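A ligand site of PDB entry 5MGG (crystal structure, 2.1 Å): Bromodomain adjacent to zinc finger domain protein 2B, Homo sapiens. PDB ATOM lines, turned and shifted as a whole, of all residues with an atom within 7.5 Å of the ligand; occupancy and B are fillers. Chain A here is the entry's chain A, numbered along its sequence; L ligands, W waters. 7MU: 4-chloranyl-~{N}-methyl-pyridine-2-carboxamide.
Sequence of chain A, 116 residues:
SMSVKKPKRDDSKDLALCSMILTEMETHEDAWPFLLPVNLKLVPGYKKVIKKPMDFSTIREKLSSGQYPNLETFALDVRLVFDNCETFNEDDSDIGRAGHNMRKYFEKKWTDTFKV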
ATOM      1  N   TRP A  32      28.524  14.259  23.579  1.00  0.00           N
ATOM      2  CA  TRP A  32      27.978  14.659  22.297  1.00  0.00           C
ATOM      3  C   TRP A  32      26.928  15.787  22.340  1.00  0.00           C
ATOM      4  O   TRP A  32      26.857  16.571  21.392  1.00  0.00           O
ATOM      5  CB  TRP A  32      27.407  13.448  21.541  1.00  0.00           C
ATOM      6  CG  TRP A  32      26.344  12.708  22.263  1.00  0.00           C
ATOM      7  CD1 TRP A  32      26.504  11.612  23.063  1.00  0.00           C
ATOM      8  CD2 TRP A  32      24.940  12.989  22.249  1.00  0.00           C
ATOM      9  NE1 TRP A  32      25.294  11.208  23.565  1.00  0.00           N
ATOM     10  CE2 TRP A  32      24.314  12.037  23.075  1.00  0.00           C
ATOM     11  CE3 TRP A  32      24.143  13.965  21.632  1.00  0.00           C
ATOM     12  CZ2 TRP A  32      22.938  12.019  23.307  1.00  0.00           C
ATOM     13  CZ3 TRP A  32      22.766  13.948  21.863  1.00  0.00           C
ATOM     14  CH2 TRP A  32      22.178  12.984  22.696  1.00  0.00           C
ATOM     15  N   PRO A  33      26.107  15.896  23.414  1.00  0.00           N
ATOM     16  CA  PRO A  33      25.178  17.026  23.306  1.00  0.00           C
ATOM     17  C   PRO A  33      25.843  18.385  23.569  1.00  0.00           C
ATOM     18  O   PRO A  33      25.175  19.406  23.406  1.00  0.00           O
ATOM     19  CB  PRO A  33      24.131  16.746  24.390  1.00  0.00           C
ATOM     20  CG  PRO A  33      24.364  15.280  24.835  1.00  0.00           C
ATOM     21  CD  PRO A  33      25.833  15.082  24.608  1.00  0.00           C
ATOM     22  N   PHE A  34      27.111  18.393  23.983  1.00  0.00           N
ATOM     23  CA  PHE A  34      27.752  19.605  24.510  1.00  0.00           C
ATOM     24  C   PHE A  34      28.983  20.073  23.743  1.00  0.00           C
ATOM     25  O   PHE A  34      29.644  21.039  24.144  1.00  0.00           O
ATOM     26  CB  PHE A  34      28.119  19.376  25.972  1.00  0.00           C
ATOM     27  CG  PHE A  34      27.031  18.696  26.764  1.00  0.00           C
ATOM     28  CD1 PHE A  34      25.855  19.382  27.074  1.00  0.00           C
ATOM     29  CD2 PHE A  34      27.161  17.354  27.163  1.00  0.00           C
ATOM     30  CE1 PHE A  34      24.841  18.757  27.778  1.00  0.00           C
ATOM     31  CE2 PHE A  34      26.143  16.722  27.871  1.00  0.00           C
ATOM     32  CZ  PHE A  34      24.980  17.412  28.179  1.00  0.00           C
ATOM     33  N   LEU A  35      29.310  19.376  22.654  1.00  0.00           N
ATOM     34  CA  LEU A  35      30.554  19.635  21.935  1.00  0.00           C
ATOM     35  C   LEU A  35      30.476  20.930  21.138  1.00  0.00           C
ATOM     36  O   LEU A  35      31.467  21.628  20.966  1.00  0.00           O
ATOM     37  CB  LEU A  35      30.898  18.463  21.027  1.00  0.00           C
ATOM     38  CG  LEU A  35      31.116  17.138  21.760  1.00  0.00           C
ATOM     39  CD1 LEU A  35      31.296  16.016  20.780  1.00  0.00           C
ATOM     40  CD2 LEU A  35      32.329  17.238  22.672  1.00  0.00           C
ATOM     41  N   LEU A  36      29.275  21.247  20.659  1.00  0.00           N
ATOM     42  CA  LEU A  36      29.047  22.400  19.804  1.00  0.00           C
ATOM     43  C   LEU A  36      27.903  23.253  20.353  1.00  0.00           C
ATOM     44  O   LEU A  36      27.067  22.752  21.102  1.00  0.00           O
ATOM     45  CB  LEU A  36      28.742  21.946  18.376  1.00  0.00           C
ATOM     46  CG  LEU A  36      29.890  21.256  17.646  1.00  0.00           C
ATOM     47  CD1 LEU A  36      29.461  21.013  16.204  1.00  0.00           C
ATOM     48  CD2 LEU A  36      31.149  22.120  17.700  1.00  0.00           C
ATOM     49  N   PRO A  37      27.858  24.541  19.983  1.00  0.00           N
ATOM     50  CA  PRO A  37      26.715  25.382  20.380  1.00  0.00           C
ATOM     51  C   PRO A  37      25.394  24.768  19.947  1.00  0.00           C
ATOM     52  O   PRO A  37      25.327  24.145  18.886  1.00  0.00           O
ATOM     53  CB  PRO A  37      26.962  26.690  19.620  1.00  0.00           C
ATOM     54  CG  PRO A  37      28.412  26.722  19.358  1.00  0.00           C
ATOM     55  CD  PRO A  37      28.833  25.288  19.167  1.00  0.00           C
ATOM     56  N   VAL A  38      24.360  24.938  20.759  1.00  0.00           N
ATOM     57  CA  VAL A  38      23.022  24.544  20.319  1.00  0.00           C
ATOM     58  C   VAL A  38      22.652  25.430  19.122  1.00  0.00           C
ATOM     59  O   VAL A  38      22.858  26.649  19.155  1.00  0.00           O
ATOM     60  CB  VAL A  38      21.989  24.654  21.462  1.00  0.00           C
ATOM     61  CG1 VAL A  38      20.567  24.617  20.905  1.00  0.00           C
ATOM     62  CG2 VAL A  38      22.212  23.544  22.498  1.00  0.00           C
ATOM     63  N   ASN A  39      22.155  24.817  18.056  1.00  0.00           N
ATOM     64  CA  ASN A  39      21.758  25.542  16.856  1.00  0.00           C
ATOM     65  C   ASN A  39      20.447  26.310  17.111  1.00  0.00           C
ATOM     66  O   ASN A  39      19.350  25.729  17.048  1.00  0.00           O
ATOM     67  CB  ASN A  39      21.605  24.574  15.678  1.00  0.00           C
ATOM     68  CG  ASN A  39      21.543  25.283  14.338  1.00  0.00           C
ATOM     69  OD1 ASN A  39      20.973  26.367  14.208  1.00  0.00           O
ATOM     70  ND2 ASN A  39      22.137  24.664  13.318  1.00  0.00           N
ATOM     71  N   LEU A  42      17.507  25.894  14.791  1.00  0.00           N
ATOM     72  CA  LEU A  42      16.930  24.579  14.584  1.00  0.00           C
ATOM     73  C   LEU A  42      16.267  24.059  15.857  1.00  0.00           C
ATOM     74  O   LEU A  42      15.507  23.103  15.817  1.00  0.00           O
ATOM     75  CB  LEU A  42      17.999  23.568  14.133  1.00  0.00           C
ATOM     76  CG  LEU A  42      18.732  23.841  12.814  1.00  0.00           C
ATOM     77  CD1 LEU A  42      19.574  22.635  12.416  1.00  0.00           C
ATOM     78  CD2 LEU A  42      17.749  24.219  11.705  1.00  0.00           C
ATOM     79  N   VAL A  43      16.568  24.686  16.983  1.00  0.00           N
ATOM     80  CA  VAL A  43      16.009  24.227  18.245  1.00  0.00           C
ATOM     81  C   VAL A  43      15.014  25.236  18.764  1.00  0.00           C
ATOM     82  O   VAL A  43      15.395  26.334  19.184  1.00  0.00           O
ATOM     83  CB  VAL A  43      17.089  23.964  19.301  1.00  0.00           C
ATOM     84  CG1 VAL A  43      16.460  23.419  20.576  1.00  0.00           C
ATOM     85  CG2 VAL A  43      18.133  22.996  18.758  1.00  0.00           C
ATOM     86  N   PRO A  44      13.732  24.861  18.725  1.00  0.00           N
ATOM     87  CA  PRO A  44      12.598  25.676  19.147  1.00  0.00           C
ATOM     88  C   PRO A  44      12.668  26.044  20.623  1.00  0.00           C
ATOM     89  O   PRO A  44      12.757  25.163  21.476  1.00  0.00           O
ATOM     90  CB  PRO A  44      11.390  24.759  18.881  1.00  0.00           C
ATOM     91  CG  PRO A  44      11.869  23.774  17.882  1.00  0.00           C
ATOM     92  CD  PRO A  44      13.308  23.545  18.232  1.00  0.00           C
ATOM     93  N   TYR A  46      14.973  27.548  22.445  1.00  0.00           N
ATOM     94  CA  TYR A  46      16.265  27.624  23.153  1.00  0.00           C
ATOM     95  C   TYR A  46      16.780  29.069  23.334  1.00  0.00           C
ATOM     96  O   TYR A  46      17.152  29.469  24.449  1.00  0.00           O
ATOM     97  CB  TYR A  46      17.330  26.806  22.436  1.00  0.00           C
ATOM     98  CG  TYR A  46      18.433  26.345  23.373  1.00  0.00           C
ATOM     99  CD1 TYR A  46      19.598  27.104  23.543  1.00  0.00           C
ATOM    100  CD2 TYR A  46      18.301  25.160  24.109  1.00  0.00           C
ATOM    101  CE1 TYR A  46      20.600  26.697  24.416  1.00  0.00           C
ATOM    102  CE2 TYR A  46      19.309  24.737  24.980  1.00  0.00           C
ATOM    103  CZ  TYR A  46      20.453  25.517  25.127  1.00  0.00           C
ATOM    104  OH  TYR A  46      21.449  25.115  25.986  1.00  0.00           O
ATOM    105  N   ILE A  50      17.120  30.047  27.192  1.00  0.00           N
ATOM    106  CA  ILE A  50      18.474  29.956  27.729  1.00  0.00           C
ATOM    107  C   ILE A  50      19.229  31.268  27.492  1.00  0.00           C
ATOM    108  O   ILE A  50      19.665  31.538  26.369  1.00  0.00           O
ATOM    109  CB  ILE A  50      19.256  28.777  27.099  1.00  0.00           C
ATOM    110  CG1 ILE A  50      18.479  27.470  27.288  1.00  0.00           C
ATOM    111  CG2 ILE A  50      20.706  28.694  27.654  1.00  0.00           C
ATOM    112  CD1 ILE A  50      18.165  27.151  28.734  1.00  0.00           C
ATOM    113  N   MET A  54      26.140  27.929  26.458  1.00  0.00           N
ATOM    114  CA  MET A  54      27.559  27.594  26.604  1.00  0.00           C
ATOM    115  C   MET A  54      27.753  26.164  26.126  1.00  0.00           C
ATOM    116  O   MET A  54      26.836  25.334  26.246  1.00  0.00           O
ATOM    117  CB  MET A  54      28.038  27.794  28.046  1.00  0.00           C
ATOM    118  CG  MET A  54      29.554  27.651  28.280  1.00  0.00           C
ATOM    119  SD  MET A  54      30.529  28.682  27.146  1.00  0.00           S
ATOM    120  CE  MET A  54      29.822  30.300  27.487  1.00  0.00           C
ATOM    121  N   ASP A  55      28.937  25.874  25.597  1.00  0.00           N
ATOM    122  CA  ASP A  55      29.256  24.536  25.113  1.00  0.00           C
ATOM    123  C   ASP A  55      30.762  24.324  25.214  1.00  0.00           C
ATOM    124  O   ASP A  55      31.505  25.284  25.423  1.00  0.00           O
ATOM    125  CB  ASP A  55      28.786  24.334  23.672  1.00  0.00           C
ATOM    126  CG  ASP A  55      29.545  25.228  22.706  1.00  0.00           C
ATOM    127  OD1 ASP A  55      29.251  26.441  22.676  1.00  0.00           O
ATOM    128  OD2 ASP A  55      30.442  24.728  21.985  1.00  0.00           O
ATOM    129  N   VAL A  81      27.006  24.974  31.302  1.00  0.00           N
ATOM    130  CA  VAL A  81      26.647  24.002  30.275  1.00  0.00           C
ATOM    131  C   VAL A  81      25.610  23.022  30.844  1.00  0.00           C
ATOM    132  O   VAL A  81      24.565  22.769  30.233  1.00  0.00           O
ATOM    133  CB  VAL A  81      27.879  23.226  29.775  1.00  0.00           C
ATOM    134  CG1 VAL A  81      27.426  22.038  28.925  1.00  0.00           C
ATOM    135  CG2 VAL A  81      28.872  24.150  28.985  1.00  0.00           C
ATOM    136  N   ASN A  84      22.253  24.818  31.931  1.00  0.00           N
ATOM    137  CA  ASN A  84      21.372  25.023  30.780  1.00  0.00           C
ATOM    138  C   ASN A  84      20.708  23.726  30.369  1.00  0.00           C
ATOM    139  O   ASN A  84      19.535  23.704  29.996  1.00  0.00           O
ATOM    140  CB  ASN A  84      22.144  25.596  29.592  1.00  0.00           C
ATOM    141  CG  ASN A  84      22.649  27.013  29.846  1.00  0.00           C
ATOM    142  OD1 ASN A  84      22.173  27.710  30.742  1.00  0.00           O
ATOM    143  ND2 ASN A  84      23.617  27.430  29.040  1.00  0.00           N
ATOM    144  N   CYS A  85      21.467  22.628  30.414  1.00  0.00           N
ATOM    145  CA  CYS A  85      20.957  21.331  30.024  1.00  0.00           C
ATOM    146  C   CYS A  85      19.777  20.920  30.908  1.00  0.00           C
ATOM    147  O   CYS A  85      18.761  20.436  30.402  1.00  0.00           O
ATOM    148  CB  CYS A  85      22.062  20.269  30.094  1.00  0.00           C
ATOM    149  SG  CYS A  85      21.555  18.635  29.515  1.00  0.00           S
ATOM    150  N   GLU A  86      19.910  21.153  32.207  1.00  0.00           N
ATOM    151  CA  GLU A  86      18.869  20.795  33.175  1.00  0.00           C
ATOM    152  C   GLU A  86      17.643  21.673  32.990  1.00  0.00           C
ATOM    153  O   GLU A  86      16.524  21.239  33.200  1.00  0.00           O
ATOM    154  CB  GLU A  86      19.354  20.936  34.603  1.00  0.00           C
ATOM    155  CG  GLU A  86      20.137  19.761  35.137  1.00  0.00           C
ATOM    156  CD  GLU A  86      20.177  19.769  36.641  1.00  0.00           C
ATOM    157  OE1 GLU A  86      21.274  19.865  37.224  1.00  0.00           O
ATOM    158  OE2 GLU A  86      19.087  19.681  37.253  1.00  0.00           O
ATOM    159  N   PHE A  88      16.547  22.899  30.212  1.00  0.00           N
ATOM    160  CA  PHE A  88      15.868  22.695  28.945  1.00  0.00           C
ATOM    161  C   PHE A  88      15.426  21.254  28.716  1.00  0.00           C
ATOM    162  O   PHE A  88      14.451  21.001  28.002  1.00  0.00           O
ATOM    163  CB  PHE A  88      16.774  23.128  27.776  1.00  0.00           C
ATOM    164  CG  PHE A  88      16.018  23.443  26.519  1.00  0.00           C
ATOM    165  CD1 PHE A  88      15.298  24.625  26.393  1.00  0.00           C
ATOM    166  CD2 PHE A  88      16.005  22.546  25.461  1.00  0.00           C
ATOM    167  CE1 PHE A  88      14.586  24.928  25.233  1.00  0.00           C
ATOM    168  CE2 PHE A  88      15.299  22.834  24.299  1.00  0.00           C
ATOM    169  CZ  PHE A  88      14.582  24.034  24.185  1.00  0.00           C
ATOM    170  N   ASN A  89      16.141  20.311  29.315  1.00  0.00           N
ATOM    171  CA  ASN A  89      15.908  18.903  29.032  1.00  0.00           C
ATOM    172  C   ASN A  89      15.347  18.164  30.243  1.00  0.00           C
ATOM    173  O   ASN A  89      15.730  18.438  31.381  1.00  0.00           O
ATOM    174  CB  ASN A  89      17.211  18.242  28.570  1.00  0.00           C
ATOM    175  CG  ASN A  89      17.794  18.890  27.318  1.00  0.00           C
ATOM    176  OD1 ASN A  89      17.392  18.561  26.199  1.00  0.00           O
ATOM    177  ND2 ASN A  89      18.762  19.798  27.486  1.00  0.00           N
ATOM    178  N   ILE A  95      19.586  13.402  26.554  1.00  0.00           N
ATOM    179  CA  ILE A  95      20.414  14.598  26.747  1.00  0.00           C
ATOM    180  C   ILE A  95      20.450  14.990  28.221  1.00  0.00           C
ATOM    181  O   ILE A  95      21.511  15.297  28.767  1.00  0.00           O
ATOM    182  CB  ILE A  95      19.908  15.780  25.900  1.00  0.00           C
ATOM    183  CG1 ILE A  95      20.031  15.451  24.413  1.00  0.00           C
ATOM    184  CG2 ILE A  95      20.705  17.048  26.224  1.00  0.00           C
ATOM    185  CD1 ILE A  95      19.540  16.548  23.511  1.00  0.00           C
ATOM    186  N   GLY A  96      19.284  14.986  28.867  1.00  0.00           N
ATOM    187  CA  GLY A  96      19.198  15.233  30.297  1.00  0.00           C
ATOM    188  C   GLY A  96      20.081  14.319  31.154  1.00  0.00           C
ATOM    189  O   GLY A  96      20.745  14.779  32.085  1.00  0.00           O
HETATM  190  C01 7MU L   1      22.856  20.632  25.296  1.00  0.00           C
HETATM  191  N02 7MU L   1      21.989  20.377  24.240  1.00  0.00           N
HETATM  192  C03 7MU L   1      20.597  20.588  24.414  1.00  0.00           C
HETATM  193  O04 7MU L   1      20.171  20.945  25.475  1.00  0.00           O
HETATM  194  C05 7MU L   1      19.730  20.269  23.245  1.00  0.00           C
HETATM  195  N06 7MU L   1      20.280  20.330  22.067  1.00  0.00           N
HETATM  196  C07 7MU L   1      19.600  20.040  20.972  1.00  0.00           C
HETATM  197  C08 7MU L   1      18.286  19.658  21.051  1.00  0.00           C
HETATM  198  C09 7MU L   1      17.675  19.571  22.290  1.00  0.00           C
HETATM  199  C10 7MU L   1      18.431  19.885  23.416  1.00  0.00           C
HETATM  200 CL   7MU L   1      16.034  19.085  22.427  1.00  0.00          CL
HETATM  201  O   HOH W   1      21.228  22.850  27.000  1.00  0.00           O
HETATM  202  O   HOH W   2      23.042  19.668  21.292  1.00  0.00           O
HETATM  203  O   HOH W   3      23.816  22.557  27.770  1.00  0.00           O
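N02 of the ligand sits close to O of Pro 33 (3.4 Å). ND2 of Asn 89 is in hydrogen-bond range of O04 of the ligand.
The backbone carbonyl oxygen of Ile 95 sits at hydrogen-bond distance from the side-chain sulfur of Cys 85, 3.4 Å away. The side-chain amide nitrogen (ND2) of Asn 89 lies within hydrogen-bond range of the backbone carbonyl oxygen (O) of Cys 85 (3.0 Å).
Phe 34 touches the ligand (CE1 to C01, 3.7 Å). CG2 of Val 38 touches N02 of the ligand, 3.6 Å away. Val 43 touches the ligand. Tyr 46 touches the ligand. Ile 95 touches the ligand (CD1 to C10, 3.5 Å). Hydrophobic or aromatic side chains that line the ligand: Phe 34, Val 38, Val 43, Tyr 46 and Ile 95. Of the 23 residues printed, 7 come within 4 Å of the ligand.
Water W1 lies within hydrogen-bond range of the side-chain hydroxyl (OH) of Tyr 46 (2.5 Å), an oxygen (O04) of the ligand (2.7 Å) and the backbone NH (N) of Cys 85 (3.4 Å). Water W2 lies within hydrogen-bond range of a nitrogen (N06) of the ligand (2.9 Å) and the backbone carbonyl oxygen (O) of Pro 33 (3.0 Å).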
